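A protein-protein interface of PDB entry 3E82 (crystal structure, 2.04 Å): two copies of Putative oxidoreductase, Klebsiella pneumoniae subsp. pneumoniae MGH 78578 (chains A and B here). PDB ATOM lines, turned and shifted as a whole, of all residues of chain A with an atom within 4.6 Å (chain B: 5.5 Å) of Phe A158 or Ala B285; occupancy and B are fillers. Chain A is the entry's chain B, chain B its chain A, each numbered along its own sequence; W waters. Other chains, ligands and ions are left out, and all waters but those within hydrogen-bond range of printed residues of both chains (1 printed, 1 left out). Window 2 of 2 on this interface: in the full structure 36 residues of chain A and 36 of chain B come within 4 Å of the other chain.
Of chain A, only Phe A158 comes within 4 Å of Ala B285.
Of the printed residues of chain A, Asp B246 touches Phe A158, Pro A160 and Leu A233.
Of the printed residues of chain A, Asp B284 touches Ala A235.
Of the printed residues of chain A, Leu B287 touches Phe A158 and Ala A235.
Of the printed residues of chain A, Gly B245 touches Phe A158 (3.9 Å).
Of the printed residues of chain B, Ala A235 touches Gly B248, Tyr B283, Asp B284 and Leu B287.
The nearest residue of chain B that does not touch Phe A158 is Gly B248 (4.1 Å).
No position is printed for both chains.
Of the 11 pairs that touch across the chains among the printed residues, none has its exchanged pair printed and touching as well.
O of Gly B245 touches CE1 of Phe A158, at 3.9 Å.
CZ of Phe A158 touches O of Asp B246, 3.6 Å away.
C of Lys B247 touches CZ of Phe A158 (3.9 Å).
Leu B287 touches Phe A158 (CD2 to CB, 3.7 Å).
Pro A160 touches Asp B246.
CD1 of Leu A233 touches CA of Asp B246, at 3.8 Å.
Gly B248 touches Ala A235 (CA to CB, 3.7 Å).
O of Tyr B283 touches CB of Ala A235 (3.8 Å).
CB of Ala A235 touches O of Asp B284, at 3.8 Å.
Leu B287 touches Ala A235 (CD2 to O, 3.4 Å).
N of Ala B285 sits at hydrogen-bond distance from O of Lys B247, 3.4 Å away.
OD1 of Asp B284 sits at hydrogen-bond distance from OG of Ser B286 (2.4 Å).
O of Arg A157 is in hydrogen-bond range of N of Leu A233 (3.2 Å).
Water W1 lies within hydrogen-bond range of the backbone carbonyl oxygen of Ala A235 (2.8 Å) and the backbone carbonyl oxygen of Leu B287 (2.8 Å).
Printed residues of chain B that touch a printed residue of chain A: Gly B245, Asp B246, Lys B247, Gly B248, Tyr B283, Asp B284, Ala B285 and Leu B287.
Hydrophobic or aromatic side chains of chain B that line the printed part of chain A: Tyr B283, Ala B285 and Leu B287.
Of the 8 printed residues of chain A, 4 touch a printed residue of chain B.
Along chain A the printed residues that touch a printed residue of chain B span positions 158 to 235.
Among the printed residues, 11 pairs touch across the chains.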
ATOM      1  N   ARG A 157      -6.388 -33.465  27.793  1.00  0.00           N
ATOM      2  CA  ARG A 157      -7.140 -32.342  28.323  1.00  0.00           C
ATOM      3  C   ARG A 157      -7.615 -31.505  27.142  1.00  0.00           C
ATOM      4  O   ARG A 157      -7.199 -31.738  26.005  1.00  0.00           O
ATOM      5  CB  ARG A 157      -6.277 -31.542  29.314  1.00  0.00           C
ATOM      6  CG  ARG A 157      -6.006 -32.370  30.572  1.00  0.00           C
ATOM      7  CD  ARG A 157      -5.383 -31.637  31.751  1.00  0.00           C
ATOM      8  NE  ARG A 157      -5.126 -32.601  32.827  1.00  0.00           N
ATOM      9  CZ  ARG A 157      -4.558 -32.314  33.998  1.00  0.00           C
ATOM     10  NH1 ARG A 157      -4.173 -31.072  34.276  1.00  0.00           N
ATOM     11  NH2 ARG A 157      -4.369 -33.276  34.898  1.00  0.00           N
ATOM     12  N   PHE A 158      -8.514 -30.565  27.394  1.00  0.00           N
ATOM     13  CA  PHE A 158      -9.030 -29.738  26.316  1.00  0.00           C
ATOM     14  C   PHE A 158      -8.597 -28.296  26.497  1.00  0.00           C
ATOM     15  O   PHE A 158      -9.112 -27.580  27.355  1.00  0.00           O
ATOM     16  CB  PHE A 158     -10.556 -29.825  26.260  1.00  0.00           C
ATOM     17  CG  PHE A 158     -11.155 -29.136  25.069  1.00  0.00           C
ATOM     18  CD1 PHE A 158     -10.909 -29.604  23.780  1.00  0.00           C
ATOM     19  CD2 PHE A 158     -11.956 -28.011  25.233  1.00  0.00           C
ATOM     20  CE1 PHE A 158     -11.455 -28.958  22.671  1.00  0.00           C
ATOM     21  CE2 PHE A 158     -12.506 -27.359  24.129  1.00  0.00           C
ATOM     22  CZ  PHE A 158     -12.256 -27.832  22.849  1.00  0.00           C
ATOM     23  N   ARG A 159      -7.635 -27.885  25.682  1.00  0.00           N
ATOM     24  CA  ARG A 159      -7.103 -26.537  25.727  1.00  0.00           C
ATOM     25  C   ARG A 159      -6.774 -26.077  24.314  1.00  0.00           C
ATOM     26  O   ARG A 159      -5.609 -26.025  23.911  1.00  0.00           O
ATOM     27  CB  ARG A 159      -5.865 -26.503  26.625  1.00  0.00           C
ATOM     28  CG  ARG A 159      -6.212 -26.764  28.088  1.00  0.00           C
ATOM     29  CD  ARG A 159      -4.995 -26.995  28.966  1.00  0.00           C
ATOM     30  NE  ARG A 159      -5.395 -27.319  30.337  1.00  0.00           N
ATOM     31  CZ  ARG A 159      -4.566 -27.766  31.277  1.00  0.00           C
ATOM     32  NH1 ARG A 159      -3.279 -27.946  30.998  1.00  0.00           N
ATOM     33  NH2 ARG A 159      -5.020 -28.034  32.498  1.00  0.00           N
ATOM     34  N   PRO A 160      -7.815 -25.735  23.540  1.00  0.00           N
ATOM     35  CA  PRO A 160      -7.664 -25.276  22.158  1.00  0.00           C
ATOM     36  C   PRO A 160      -6.913 -23.950  22.077  1.00  0.00           C
ATOM     37  O   PRO A 160      -6.247 -23.657  21.080  1.00  0.00           O
ATOM     38  CB  PRO A 160      -9.108 -25.162  21.680  1.00  0.00           C
ATOM     39  CG  PRO A 160      -9.828 -24.743  22.930  1.00  0.00           C
ATOM     40  CD  PRO A 160      -9.227 -25.674  23.959  1.00  0.00           C
ATOM     41  N   MET A 232      -3.619 -32.223  23.928  1.00  0.00           N
ATOM     42  CA  MET A 232      -4.185 -31.023  24.534  1.00  0.00           C
ATOM     43  C   MET A 232      -5.557 -30.709  23.931  1.00  0.00           C
ATOM     44  O   MET A 232      -6.185 -29.711  24.285  1.00  0.00           O
ATOM     45  CB  MET A 232      -3.250 -29.828  24.319  1.00  0.00           C
ATOM     46  CG  MET A 232      -1.905 -29.974  25.010  1.00  0.00           C
ATOM     47  SD  MET A 232      -2.134 -30.057  26.926  1.00  0.00           S
ATOM     48  CE  MET A 232      -1.411 -28.311  27.386  1.00  0.00           C
ATOM     49  N   LEU A 233      -6.025 -31.555  23.019  1.00  0.00           N
ATOM     50  CA  LEU A 233      -7.327 -31.323  22.400  1.00  0.00           C
ATOM     51  C   LEU A 233      -8.291 -32.486  22.484  1.00  0.00           C
ATOM     52  O   LEU A 233      -8.592 -33.130  21.483  1.00  0.00           O
ATOM     53  CB  LEU A 233      -7.170 -30.922  20.937  1.00  0.00           C
ATOM     54  CG  LEU A 233      -7.030 -29.427  20.669  1.00  0.00           C
ATOM     55  CD1 LEU A 233      -7.166 -29.194  19.183  1.00  0.00           C
ATOM     56  CD2 LEU A 233      -8.102 -28.643  21.423  1.00  0.00           C
ATOM     57  N   VAL A 234      -8.781 -32.744  23.687  1.00  0.00           N
ATOM     58  CA  VAL A 234      -9.733 -33.820  23.906  1.00  0.00           C
ATOM     59  C   VAL A 234     -10.853 -33.267  24.775  1.00  0.00           C
ATOM     60  O   VAL A 234     -10.731 -33.216  25.997  1.00  0.00           O
ATOM     61  CB  VAL A 234      -9.075 -35.027  24.621  1.00  0.00           C
ATOM     62  CG1 VAL A 234     -10.111 -36.121  24.866  1.00  0.00           C
ATOM     63  CG2 VAL A 234      -7.934 -35.571  23.775  1.00  0.00           C
ATOM     64  N   ALA A 235     -11.937 -32.840  24.137  1.00  0.00           N
ATOM     65  CA  ALA A 235     -13.075 -32.283  24.857  1.00  0.00           C
ATOM     66  C   ALA A 235     -13.748 -33.355  25.696  1.00  0.00           C
ATOM     67  O   ALA A 235     -14.361 -33.050  26.717  1.00  0.00           O
ATOM     68  CB  ALA A 235     -14.076 -31.676  23.879  1.00  0.00           C
ATOM     69  N   GLY B 245     -11.738 -32.433  17.631  1.00  0.00           N
ATOM     70  CA  GLY B 245     -11.497 -31.236  16.843  1.00  0.00           C
ATOM     71  C   GLY B 245     -11.184 -30.125  17.837  1.00  0.00           C
ATOM     72  O   GLY B 245     -11.218 -30.361  19.047  1.00  0.00           O
ATOM     73  N   ASP B 246     -10.885 -28.919  17.369  1.00  0.00           N
ATOM     74  CA  ASP B 246     -10.577 -27.849  18.315  1.00  0.00           C
ATOM     75  C   ASP B 246     -11.806 -27.179  18.928  1.00  0.00           C
ATOM     76  O   ASP B 246     -11.673 -26.238  19.704  1.00  0.00           O
ATOM     77  CB  ASP B 246      -9.668 -26.793  17.675  1.00  0.00           C
ATOM     78  CG  ASP B 246     -10.117 -26.392  16.294  1.00  0.00           C
ATOM     79  OD1 ASP B 246     -11.341 -26.337  16.058  1.00  0.00           O
ATOM     80  OD2 ASP B 246      -9.241 -26.121  15.445  1.00  0.00           O
ATOM     81  N   LYS B 247     -13.001 -27.655  18.585  1.00  0.00           N
ATOM     82  CA  LYS B 247     -14.217 -27.090  19.165  1.00  0.00           C
ATOM     83  C   LYS B 247     -14.955 -28.134  19.997  1.00  0.00           C
ATOM     84  O   LYS B 247     -15.843 -27.799  20.783  1.00  0.00           O
ATOM     85  CB  LYS B 247     -15.162 -26.548  18.083  1.00  0.00           C
ATOM     86  CG  LYS B 247     -14.680 -25.280  17.404  1.00  0.00           C
ATOM     87  CD  LYS B 247     -15.735 -24.701  16.467  1.00  0.00           C
ATOM     88  CE  LYS B 247     -16.997 -24.323  17.229  1.00  0.00           C
ATOM     89  NZ  LYS B 247     -17.949 -23.524  16.399  1.00  0.00           N
ATOM     90  N   GLY B 248     -14.586 -29.399  19.825  1.00  0.00           N
ATOM     91  CA  GLY B 248     -15.243 -30.455  20.574  1.00  0.00           C
ATOM     92  C   GLY B 248     -14.934 -31.847  20.048  1.00  0.00           C
ATOM     93  O   GLY B 248     -14.179 -32.010  19.081  1.00  0.00           O
ATOM     94  N   TYR B 283     -19.221 -33.799  22.818  1.00  0.00           N
ATOM     95  CA  TYR B 283     -18.669 -32.993  23.902  1.00  0.00           C
ATOM     96  C   TYR B 283     -18.292 -31.632  23.322  1.00  0.00           C
ATOM     97  O   TYR B 283     -17.527 -31.563  22.359  1.00  0.00           O
ATOM     98  CB  TYR B 283     -17.413 -33.668  24.463  1.00  0.00           C
ATOM     99  CG  TYR B 283     -17.664 -35.011  25.111  1.00  0.00           C
ATOM    100  CD1 TYR B 283     -18.000 -35.103  26.464  1.00  0.00           C
ATOM    101  CD2 TYR B 283     -17.573 -36.193  24.372  1.00  0.00           C
ATOM    102  CE1 TYR B 283     -18.234 -36.343  27.067  1.00  0.00           C
ATOM    103  CE2 TYR B 283     -17.809 -37.429  24.963  1.00  0.00           C
ATOM    104  CZ  TYR B 283     -18.136 -37.497  26.309  1.00  0.00           C
ATOM    105  OH  TYR B 283     -18.357 -38.721  26.893  1.00  0.00           O
ATOM    106  N   ASP B 284     -18.833 -30.551  23.880  1.00  0.00           N
ATOM    107  CA  ASP B 284     -18.493 -29.221  23.382  1.00  0.00           C
ATOM    108  C   ASP B 284     -17.361 -28.645  24.229  1.00  0.00           C
ATOM    109  O   ASP B 284     -16.826 -29.329  25.111  1.00  0.00           O
ATOM    110  CB  ASP B 284     -19.708 -28.283  23.407  1.00  0.00           C
ATOM    111  CG  ASP B 284     -20.328 -28.165  24.782  1.00  0.00           C
ATOM    112  OD1 ASP B 284     -19.572 -28.134  25.770  1.00  0.00           O
ATOM    113  OD2 ASP B 284     -21.572 -28.094  24.876  1.00  0.00           O
ATOM    114  N   ALA B 285     -16.998 -27.393  23.962  1.00  0.00           N
ATOM    115  CA  ALA B 285     -15.915 -26.731  24.686  1.00  0.00           C
ATOM    116  C   ALA B 285     -16.121 -26.693  26.199  1.00  0.00           C
ATOM    117  O   ALA B 285     -15.184 -26.412  26.949  1.00  0.00           O
ATOM    118  CB  ALA B 285     -15.722 -25.318  24.151  1.00  0.00           C
ATOM    119  N   SER B 286     -17.340 -26.978  26.646  1.00  0.00           N
ATOM    120  CA  SER B 286     -17.649 -26.969  28.074  1.00  0.00           C
ATOM    121  C   SER B 286     -17.431 -28.346  28.690  1.00  0.00           C
ATOM    122  O   SER B 286     -17.719 -28.557  29.869  1.00  0.00           O
ATOM    123  CB  SER B 286     -19.100 -26.544  28.304  1.00  0.00           C
ATOM    124  OG  SER B 286     -19.985 -27.633  28.085  1.00  0.00           O
ATOM    125  N   LEU B 287     -16.937 -29.281  27.879  1.00  0.00           N
ATOM    126  CA  LEU B 287     -16.662 -30.649  28.317  1.00  0.00           C
ATOM    127  C   LEU B 287     -17.926 -31.429  28.647  1.00  0.00           C
ATOM    128  O   LEU B 287     -17.859 -32.558  29.141  1.00  0.00           O
ATOM    129  CB  LEU B 287     -15.741 -30.646  29.538  1.00  0.00           C
ATOM    130  CG  LEU B 287     -14.514 -29.739  29.457  1.00  0.00           C
ATOM    131  CD1 LEU B 287     -13.685 -29.888  30.728  1.00  0.00           C
ATOM    132  CD2 LEU B 287     -13.696 -30.089  28.226  1.00  0.00           C
HETATM  133  O   HOH W   1     -15.608 -34.235  28.908  1.00  0.00           O
